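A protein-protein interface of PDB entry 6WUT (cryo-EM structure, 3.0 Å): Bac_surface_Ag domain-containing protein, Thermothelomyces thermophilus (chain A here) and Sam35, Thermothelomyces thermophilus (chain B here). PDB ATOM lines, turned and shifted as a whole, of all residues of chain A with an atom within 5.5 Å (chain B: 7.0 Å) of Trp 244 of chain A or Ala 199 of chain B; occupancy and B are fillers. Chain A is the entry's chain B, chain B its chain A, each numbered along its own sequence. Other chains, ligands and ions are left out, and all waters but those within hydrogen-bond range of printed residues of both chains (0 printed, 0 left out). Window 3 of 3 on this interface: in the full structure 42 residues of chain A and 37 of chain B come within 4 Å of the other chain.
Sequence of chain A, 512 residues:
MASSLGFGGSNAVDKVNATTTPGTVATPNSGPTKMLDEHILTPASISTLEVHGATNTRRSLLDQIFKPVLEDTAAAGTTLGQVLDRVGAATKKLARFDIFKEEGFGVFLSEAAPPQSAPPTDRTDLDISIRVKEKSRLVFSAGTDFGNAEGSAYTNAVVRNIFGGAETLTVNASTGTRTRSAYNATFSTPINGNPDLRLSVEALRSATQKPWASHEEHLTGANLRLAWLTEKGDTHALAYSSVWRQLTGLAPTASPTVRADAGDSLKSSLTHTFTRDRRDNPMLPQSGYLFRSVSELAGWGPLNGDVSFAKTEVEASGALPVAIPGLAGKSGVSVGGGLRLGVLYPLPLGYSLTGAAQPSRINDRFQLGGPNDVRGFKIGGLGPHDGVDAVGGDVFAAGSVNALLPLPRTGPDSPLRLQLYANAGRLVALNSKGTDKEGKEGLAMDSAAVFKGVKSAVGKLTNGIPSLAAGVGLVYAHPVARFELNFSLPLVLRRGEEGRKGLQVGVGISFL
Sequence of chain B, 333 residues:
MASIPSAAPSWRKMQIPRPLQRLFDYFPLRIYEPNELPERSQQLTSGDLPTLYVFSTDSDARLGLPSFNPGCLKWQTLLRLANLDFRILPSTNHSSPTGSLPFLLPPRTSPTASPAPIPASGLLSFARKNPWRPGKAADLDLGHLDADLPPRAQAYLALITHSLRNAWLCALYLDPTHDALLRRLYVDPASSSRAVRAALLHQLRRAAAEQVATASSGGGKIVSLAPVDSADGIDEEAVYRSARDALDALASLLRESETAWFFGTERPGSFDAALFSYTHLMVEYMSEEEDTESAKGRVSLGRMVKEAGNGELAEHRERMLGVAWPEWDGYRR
Printed residues of chain B that touch a printed residue of chain A: Ser 193, Val 196, Ala 199 and Leu 200. Hydrophobic or aromatic side chains of chain B that line the printed part of chain A: Val 196, Ala 199 and Leu 200. Hydrophobic or aromatic side chains of chain A within 4 Å of the printed part of chain B: Trp 244 and Leu 266. Among the printed residues, 5 pairs touch across the chains.
NE1 of Trp 244 of chain A touches CG1 of Val 196 of chain B, 3.4 Å away. Trp 244 of chain A touches Ala 199 of chain B (CH2 to CB, 3.6 Å). Leu 200 of chain B touches Asp 264 of chain A (CD1 to OD2, 3.3 Å). OG of Ser 193 of chain B touches CD1 of Leu 266 of chain A, 3.6 Å away. Leu 266 of chain A touches Val 196 of chain B.
O of Trp 244 of chain A lies within hydrogen-bond range of N of Ser 265 of chain A. The backbone NH of Val 243 of chain A sits close to the backbone carbonyl oxygen of Leu 266 of chain A, 3.4 Å away. The backbone NH (N) of Trp 244 of chain A lies within hydrogen-bond range of the backbone carbonyl oxygen (O) of Thr 220 of chain A (3.1 Å).
Val 243 of chain A touches none of the printed residues of chain B. Of chain B, only Val 196 (3.4 Å) and Ala 199 (3.6 Å) come within 4 Å of Trp 244 of chain A. Of the printed residues of chain B, Asp 264 of chain A touches Leu 200 (3.3 Å). Printed residues of chain B within 4 Å of Leu 266 of chain A: Ser 193 and Val 196. Printed residues of chain A within 4 Å of Ser 193 of chain B: Leu 266. Printed residues of chain A within 4 Å of Ala 199 of chain B: Trp 244 (3.6 Å). Printed residues of chain A within 4 Å of Leu 200 of chain B: Asp 264 (3.3 Å). The nearest residue of chain B that does not touch Trp 244 of chain A is Leu 200 of chain B (4.1 Å). The nearest printed residue of chain A that does not touch Ala 199 of chain B is Thr 220 of chain A (7.9 Å).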
ATOM      1  N   HIS A 218     -15.827  21.734  19.719  1.00  0.00           N
ATOM      2  CA  HIS A 218     -14.928  20.747  19.141  1.00  0.00           C
ATOM      3  C   HIS A 218     -15.590  20.179  17.899  1.00  0.00           C
ATOM      4  O   HIS A 218     -16.596  19.475  18.004  1.00  0.00           O
ATOM      5  CB  HIS A 218     -14.631  19.629  20.135  1.00  0.00           C
ATOM      6  CG  HIS A 218     -13.829  20.056  21.324  1.00  0.00           C
ATOM      7  ND1 HIS A 218     -13.206  19.150  22.152  1.00  0.00           N
ATOM      8  CD2 HIS A 218     -13.545  21.279  21.826  1.00  0.00           C
ATOM      9  CE1 HIS A 218     -12.572  19.798  23.111  1.00  0.00           C
ATOM     10  NE2 HIS A 218     -12.761  21.092  22.935  1.00  0.00           N
ATOM     11  N   LEU A 219     -15.026  20.466  16.731  1.00  0.00           N
ATOM     12  CA  LEU A 219     -15.639  20.141  15.448  1.00  0.00           C
ATOM     13  C   LEU A 219     -14.776  19.116  14.732  1.00  0.00           C
ATOM     14  O   LEU A 219     -13.699  19.456  14.252  1.00  0.00           O
ATOM     15  CB  LEU A 219     -15.776  21.390  14.585  1.00  0.00           C
ATOM     16  CG  LEU A 219     -16.621  22.549  15.081  1.00  0.00           C
ATOM     17  CD1 LEU A 219     -16.399  23.748  14.206  1.00  0.00           C
ATOM     18  CD2 LEU A 219     -18.048  22.146  15.019  1.00  0.00           C
ATOM     19  N   THR A 220     -15.241  17.875  14.640  1.00  0.00           N
ATOM     20  CA  THR A 220     -14.591  16.866  13.812  1.00  0.00           C
ATOM     21  C   THR A 220     -15.555  16.390  12.736  1.00  0.00           C
ATOM     22  O   THR A 220     -16.673  15.973  13.045  1.00  0.00           O
ATOM     23  CB  THR A 220     -14.120  15.656  14.625  1.00  0.00           C
ATOM     24  OG1 THR A 220     -15.205  14.743  14.792  1.00  0.00           O
ATOM     25  CG2 THR A 220     -13.615  16.070  15.984  1.00  0.00           C
ATOM     26  N   GLY A 221     -15.119  16.429  11.484  1.00  0.00           N
ATOM     27  CA  GLY A 221     -15.927  15.850  10.431  1.00  0.00           C
ATOM     28  C   GLY A 221     -15.282  16.014   9.075  1.00  0.00           C
ATOM     29  O   GLY A 221     -14.138  16.441   8.963  1.00  0.00           O
ATOM     30  N   SER A 242     -20.599  17.188   7.153  1.00  0.00           N
ATOM     31  CA  SER A 242     -21.033  16.327   8.250  1.00  0.00           C
ATOM     32  C   SER A 242     -20.055  16.510   9.399  1.00  0.00           C
ATOM     33  O   SER A 242     -18.877  16.202   9.240  1.00  0.00           O
ATOM     34  CB  SER A 242     -21.084  14.869   7.818  1.00  0.00           C
ATOM     35  OG  SER A 242     -21.732  14.086   8.798  1.00  0.00           O
ATOM     36  N   VAL A 243     -20.533  17.008  10.544  1.00  0.00           N
ATOM     37  CA  VAL A 243     -19.669  17.420  11.651  1.00  0.00           C
ATOM     38  C   VAL A 243     -20.030  16.630  12.905  1.00  0.00           C
ATOM     39  O   VAL A 243     -20.807  15.678  12.835  1.00  0.00           O
ATOM     40  CB  VAL A 243     -19.752  18.934  11.915  1.00  0.00           C
ATOM     41  CG1 VAL A 243     -18.363  19.518  12.091  1.00  0.00           C
ATOM     42  CG2 VAL A 243     -20.484  19.662  10.808  1.00  0.00           C
ATOM     43  N   TRP A 244     -19.408  16.948  14.039  1.00  0.00           N
ATOM     44  CA  TRP A 244     -19.804  16.387  15.325  1.00  0.00           C
ATOM     45  C   TRP A 244     -20.297  17.465  16.280  1.00  0.00           C
ATOM     46  O   TRP A 244     -21.358  17.291  16.883  1.00  0.00           O
ATOM     47  CB  TRP A 244     -18.642  15.576  15.935  1.00  0.00           C
ATOM     48  CG  TRP A 244     -18.885  14.767  17.249  1.00  0.00           C
ATOM     49  CD1 TRP A 244     -19.889  14.919  18.169  1.00  0.00           C
ATOM     50  CD2 TRP A 244     -18.053  13.719  17.760  1.00  0.00           C
ATOM     51  NE1 TRP A 244     -19.734  14.042  19.200  1.00  0.00           N
ATOM     52  CE2 TRP A 244     -18.614  13.294  18.977  1.00  0.00           C
ATOM     53  CE3 TRP A 244     -16.889  13.100  17.307  1.00  0.00           C
ATOM     54  CZ2 TRP A 244     -18.058  12.273  19.733  1.00  0.00           C
ATOM     55  CZ3 TRP A 244     -16.339  12.091  18.062  1.00  0.00           C
ATOM     56  CH2 TRP A 244     -16.922  11.688  19.260  1.00  0.00           C
ATOM     57  N   ARG A 245     -19.581  18.587  16.412  1.00  0.00           N
ATOM     58  CA  ARG A 245     -20.008  19.778  17.165  1.00  0.00           C
ATOM     59  C   ARG A 245     -20.274  19.464  18.641  1.00  0.00           C
ATOM     60  O   ARG A 245     -21.403  19.493  19.116  1.00  0.00           O
ATOM     61  CB  ARG A 245     -21.244  20.452  16.546  1.00  0.00           C
ATOM     62  CG  ARG A 245     -21.307  20.479  15.044  1.00  0.00           C
ATOM     63  CD  ARG A 245     -22.504  21.225  14.573  1.00  0.00           C
ATOM     64  NE  ARG A 245     -23.697  20.862  15.312  1.00  0.00           N
ATOM     65  CZ  ARG A 245     -24.822  21.552  15.257  1.00  0.00           C
ATOM     66  NH1 ARG A 245     -24.884  22.628  14.497  1.00  0.00           N
ATOM     67  NH2 ARG A 245     -25.879  21.177  15.952  1.00  0.00           N
ATOM     68  N   GLN A 246     -19.202  19.159  19.356  1.00  0.00           N
ATOM     69  CA  GLN A 246     -19.272  18.927  20.793  1.00  0.00           C
ATOM     70  C   GLN A 246     -19.049  20.230  21.553  1.00  0.00           C
ATOM     71  O   GLN A 246     -18.009  20.869  21.396  1.00  0.00           O
ATOM     72  CB  GLN A 246     -18.243  17.885  21.208  1.00  0.00           C
ATOM     73  CG  GLN A 246     -18.073  17.757  22.691  1.00  0.00           C
ATOM     74  CD  GLN A 246     -17.630  16.376  23.097  1.00  0.00           C
ATOM     75  OE1 GLN A 246     -16.680  16.217  23.858  1.00  0.00           O
ATOM     76  NE2 GLN A 246     -18.318  15.366  22.589  1.00  0.00           N
ATOM     77  N   ASP A 264     -23.337  16.697  22.366  1.00  0.00           N
ATOM     78  CA  ASP A 264     -22.972  16.213  21.047  1.00  0.00           C
ATOM     79  C   ASP A 264     -24.114  16.382  20.055  1.00  0.00           C
ATOM     80  O   ASP A 264     -25.289  16.261  20.404  1.00  0.00           O
ATOM     81  CB  ASP A 264     -22.561  14.747  21.130  1.00  0.00           C
ATOM     82  CG  ASP A 264     -21.644  14.476  22.298  1.00  0.00           C
ATOM     83  OD1 ASP A 264     -20.698  15.256  22.506  1.00  0.00           O
ATOM     84  OD2 ASP A 264     -21.882  13.497  23.026  1.00  0.00           O
ATOM     85  N   SER A 265     -23.747  16.664  18.805  1.00  0.00           N
ATOM     86  CA  SER A 265     -24.683  16.856  17.708  1.00  0.00           C
ATOM     87  C   SER A 265     -24.204  16.041  16.512  1.00  0.00           C
ATOM     88  O   SER A 265     -23.250  15.271  16.617  1.00  0.00           O
ATOM     89  CB  SER A 265     -24.806  18.339  17.377  1.00  0.00           C
ATOM     90  OG  SER A 265     -25.753  18.969  18.212  1.00  0.00           O
ATOM     91  N   LEU A 266     -24.906  16.128  15.382  1.00  0.00           N
ATOM     92  CA  LEU A 266     -24.295  15.716  14.124  1.00  0.00           C
ATOM     93  C   LEU A 266     -24.253  16.832  13.089  1.00  0.00           C
ATOM     94  O   LEU A 266     -23.158  17.209  12.663  1.00  0.00           O
ATOM     95  CB  LEU A 266     -24.993  14.490  13.537  1.00  0.00           C
ATOM     96  CG  LEU A 266     -24.200  13.876  12.382  1.00  0.00           C
ATOM     97  CD1 LEU A 266     -22.943  13.254  12.887  1.00  0.00           C
ATOM     98  CD2 LEU A 266     -25.005  12.843  11.651  1.00  0.00           C
ATOM     99  N   VAL B 187     -25.656   6.209  25.723  1.00  0.00           N
ATOM    100  CA  VAL B 187     -25.163   6.460  24.382  1.00  0.00           C
ATOM    101  C   VAL B 187     -26.288   6.830  23.426  1.00  0.00           C
ATOM    102  O   VAL B 187     -26.148   7.757  22.626  1.00  0.00           O
ATOM    103  CB  VAL B 187     -24.367   5.231  23.888  1.00  0.00           C
ATOM    104  CG1 VAL B 187     -23.997   5.350  22.463  1.00  0.00           C
ATOM    105  CG2 VAL B 187     -23.112   5.077  24.709  1.00  0.00           C
ATOM    106  N   SER B 191     -26.901  11.065  20.960  1.00  0.00           N
ATOM    107  CA  SER B 191     -27.142  11.423  19.566  1.00  0.00           C
ATOM    108  C   SER B 191     -27.808  10.239  18.880  1.00  0.00           C
ATOM    109  O   SER B 191     -28.061   9.202  19.497  1.00  0.00           O
ATOM    110  CB  SER B 191     -25.849  11.806  18.846  1.00  0.00           C
ATOM    111  OG  SER B 191     -24.996  10.689  18.749  1.00  0.00           O
ATOM    112  N   SER B 193     -26.557   9.295  15.597  1.00  0.00           N
ATOM    113  CA  SER B 193     -25.635   8.864  14.561  1.00  0.00           C
ATOM    114  C   SER B 193     -24.750   7.758  15.097  1.00  0.00           C
ATOM    115  O   SER B 193     -24.228   7.861  16.206  1.00  0.00           O
ATOM    116  CB  SER B 193     -24.774  10.025  14.079  1.00  0.00           C
ATOM    117  OG  SER B 193     -24.365  10.817  15.171  1.00  0.00           O
ATOM    118  N   ARG B 194     -24.566   6.710  14.291  1.00  0.00           N
ATOM    119  CA  ARG B 194     -23.884   5.512  14.762  1.00  0.00           C
ATOM    120  C   ARG B 194     -22.396   5.736  14.966  1.00  0.00           C
ATOM    121  O   ARG B 194     -21.790   5.075  15.814  1.00  0.00           O
ATOM    122  CB  ARG B 194     -24.105   4.365  13.783  1.00  0.00           C
ATOM    123  CG  ARG B 194     -25.558   4.115  13.459  1.00  0.00           C
ATOM    124  CD  ARG B 194     -25.807   2.654  13.170  1.00  0.00           C
ATOM    125  NE  ARG B 194     -25.039   2.179  12.026  1.00  0.00           N
ATOM    126  CZ  ARG B 194     -25.557   1.953  10.824  1.00  0.00           C
ATOM    127  NH1 ARG B 194     -26.848   2.159  10.611  1.00  0.00           N
ATOM    128  NH2 ARG B 194     -24.785   1.520   9.837  1.00  0.00           N
ATOM    129  N   ALA B 195     -21.794   6.655  14.215  1.00  0.00           N
ATOM    130  CA  ALA B 195     -20.372   6.936  14.382  1.00  0.00           C
ATOM    131  C   ALA B 195     -20.111   7.666  15.689  1.00  0.00           C
ATOM    132  O   ALA B 195     -19.191   7.313  16.436  1.00  0.00           O
ATOM    133  CB  ALA B 195     -19.857   7.748  13.199  1.00  0.00           C
ATOM    134  N   VAL B 196     -20.929   8.677  15.987  1.00  0.00           N
ATOM    135  CA  VAL B 196     -20.823   9.407  17.244  1.00  0.00           C
ATOM    136  C   VAL B 196     -21.176   8.501  18.413  1.00  0.00           C
ATOM    137  O   VAL B 196     -20.513   8.532  19.453  1.00  0.00           O
ATOM    138  CB  VAL B 196     -21.718  10.658  17.192  1.00  0.00           C
ATOM    139  CG1 VAL B 196     -21.746  11.382  18.523  1.00  0.00           C
ATOM    140  CG2 VAL B 196     -21.257  11.591  16.095  1.00  0.00           C
ATOM    141  N   ARG B 197     -22.184   7.639  18.235  1.00  0.00           N
ATOM    142  CA  ARG B 197     -22.576   6.687  19.271  1.00  0.00           C
ATOM    143  C   ARG B 197     -21.450   5.711  19.594  1.00  0.00           C
ATOM    144  O   ARG B 197     -21.138   5.468  20.766  1.00  0.00           O
ATOM    145  CB  ARG B 197     -23.815   5.918  18.827  1.00  0.00           C
ATOM    146  CG  ARG B 197     -25.117   6.607  19.093  1.00  0.00           C
ATOM    147  CD  ARG B 197     -26.261   5.757  18.638  1.00  0.00           C
ATOM    148  NE  ARG B 197     -27.536   6.350  19.003  1.00  0.00           N
ATOM    149  CZ  ARG B 197     -28.704   5.908  18.568  1.00  0.00           C
ATOM    150  NH1 ARG B 197     -28.753   4.875  17.744  1.00  0.00           N
ATOM    151  NH2 ARG B 197     -29.822   6.497  18.951  1.00  0.00           N
ATOM    152  N   ALA B 198     -20.809   5.169  18.555  1.00  0.00           N
ATOM    153  CA  ALA B 198     -19.715   4.225  18.741  1.00  0.00           C
ATOM    154  C   ALA B 198     -18.506   4.891  19.381  1.00  0.00           C
ATOM    155  O   ALA B 198     -17.858   4.300  20.256  1.00  0.00           O
ATOM    156  CB  ALA B 198     -19.337   3.608  17.402  1.00  0.00           C
ATOM    157  N   ALA B 199     -18.211   6.134  18.990  1.00  0.00           N
ATOM    158  CA  ALA B 199     -17.071   6.833  19.572  1.00  0.00           C
ATOM    159  C   ALA B 199     -17.313   7.198  21.032  1.00  0.00           C
ATOM    160  O   ALA B 199     -16.395   7.108  21.858  1.00  0.00           O
ATOM    161  CB  ALA B 199     -16.761   8.082  18.756  1.00  0.00           C
ATOM    162  N   LEU B 200     -18.544   7.586  21.378  1.00  0.00           N
ATOM    163  CA  LEU B 200     -18.860   7.912  22.766  1.00  0.00           C
ATOM    164  C   LEU B 200     -18.838   6.678  23.650  1.00  0.00           C
ATOM    165  O   LEU B 200     -18.373   6.741  24.794  1.00  0.00           O
ATOM    166  CB  LEU B 200     -20.224   8.579  22.856  1.00  0.00           C
ATOM    167  CG  LEU B 200     -20.336   9.998  22.340  1.00  0.00           C
ATOM    168  CD1 LEU B 200     -21.796  10.292  22.181  1.00  0.00           C
ATOM    169  CD2 LEU B 200     -19.675  10.969  23.279  1.00  0.00           C
ATOM    170  N   LEU B 201     -19.332   5.549  23.138  1.00  0.00           N
ATOM    171  CA  LEU B 201     -19.273   4.300  23.889  1.00  0.00           C
ATOM    172  C   LEU B 201     -17.831   3.847  24.106  1.00  0.00           C
ATOM    173  O   LEU B 201     -17.489   3.329  25.179  1.00  0.00           O
ATOM    174  CB  LEU B 201     -20.079   3.236  23.155  1.00  0.00           C
ATOM    175  CG  LEU B 201     -20.258   1.877  23.805  1.00  0.00           C
ATOM    176  CD1 LEU B 201     -21.146   1.963  25.015  1.00  0.00           C
ATOM    177  CD2 LEU B 201     -20.851   0.950  22.797  1.00  0.00           C
ATOM    178  N   HIS B 202     -16.963   4.075  23.113  1.00  0.00           N
ATOM    179  CA  HIS B 202     -15.547   3.763  23.274  1.00  0.00           C
ATOM    180  C   HIS B 202     -14.886   4.632  24.334  1.00  0.00           C
ATOM    181  O   HIS B 202     -14.086   4.130  25.134  1.00  0.00           O
ATOM    182  CB  HIS B 202     -14.816   3.921  21.948  1.00  0.00           C
ATOM    183  CG  HIS B 202     -13.332   3.788  22.063  1.00  0.00           C
ATOM    184  ND1 HIS B 202     -12.711   2.594  22.355  1.00  0.00           N
ATOM    185  CD2 HIS B 202     -12.345   4.706  21.945  1.00  0.00           C
ATOM    186  CE1 HIS B 202     -11.405   2.780  22.398  1.00  0.00           C
ATOM    187  NE2 HIS B 202     -11.157   4.054  22.159  1.00  0.00           N
ATOM    188  N   GLN B 203     -15.189   5.933  24.351  1.00  0.00           N
ATOM    189  CA  GLN B 203     -14.608   6.800  25.375  1.00  0.00           C
ATOM    190  C   GLN B 203     -15.120   6.458  26.770  1.00  0.00           C
ATOM    191  O   GLN B 203     -14.358   6.543  27.741  1.00  0.00           O
ATOM    192  CB  GLN B 203     -14.894   8.268  25.068  1.00  0.00           C
ATOM    193  CG  GLN B 203     -14.348   8.785  23.739  1.00  0.00           C
ATOM    194  CD  GLN B 203     -12.874   8.491  23.525  1.00  0.00           C
ATOM    195  OE1 GLN B 203     -12.044   8.717  24.405  1.00  0.00           O
ATOM    196  NE2 GLN B 203     -12.542   7.990  22.339  1.00  0.00           N
ATOM    197  N   LEU B 204     -16.386   6.045  26.882  1.00  0.00           N
ATOM    198  CA  LEU B 204     -16.940   5.628  28.169  1.00  0.00           C
ATOM    199  C   LEU B 204     -16.238   4.389  28.698  1.00  0.00           C
ATOM    200  O   LEU B 204     -15.871   4.324  29.878  1.00  0.00           O
ATOM    201  CB  LEU B 204     -18.432   5.351  28.029  1.00  0.00           C
ATOM    202  CG  LEU B 204     -19.426   6.496  27.967  1.00  0.00           C
ATOM    203  CD1 LEU B 204     -20.752   5.918  27.572  1.00  0.00           C
ATOM    204  CD2 LEU B 204     -19.539   7.174  29.298  1.00  0.00           C
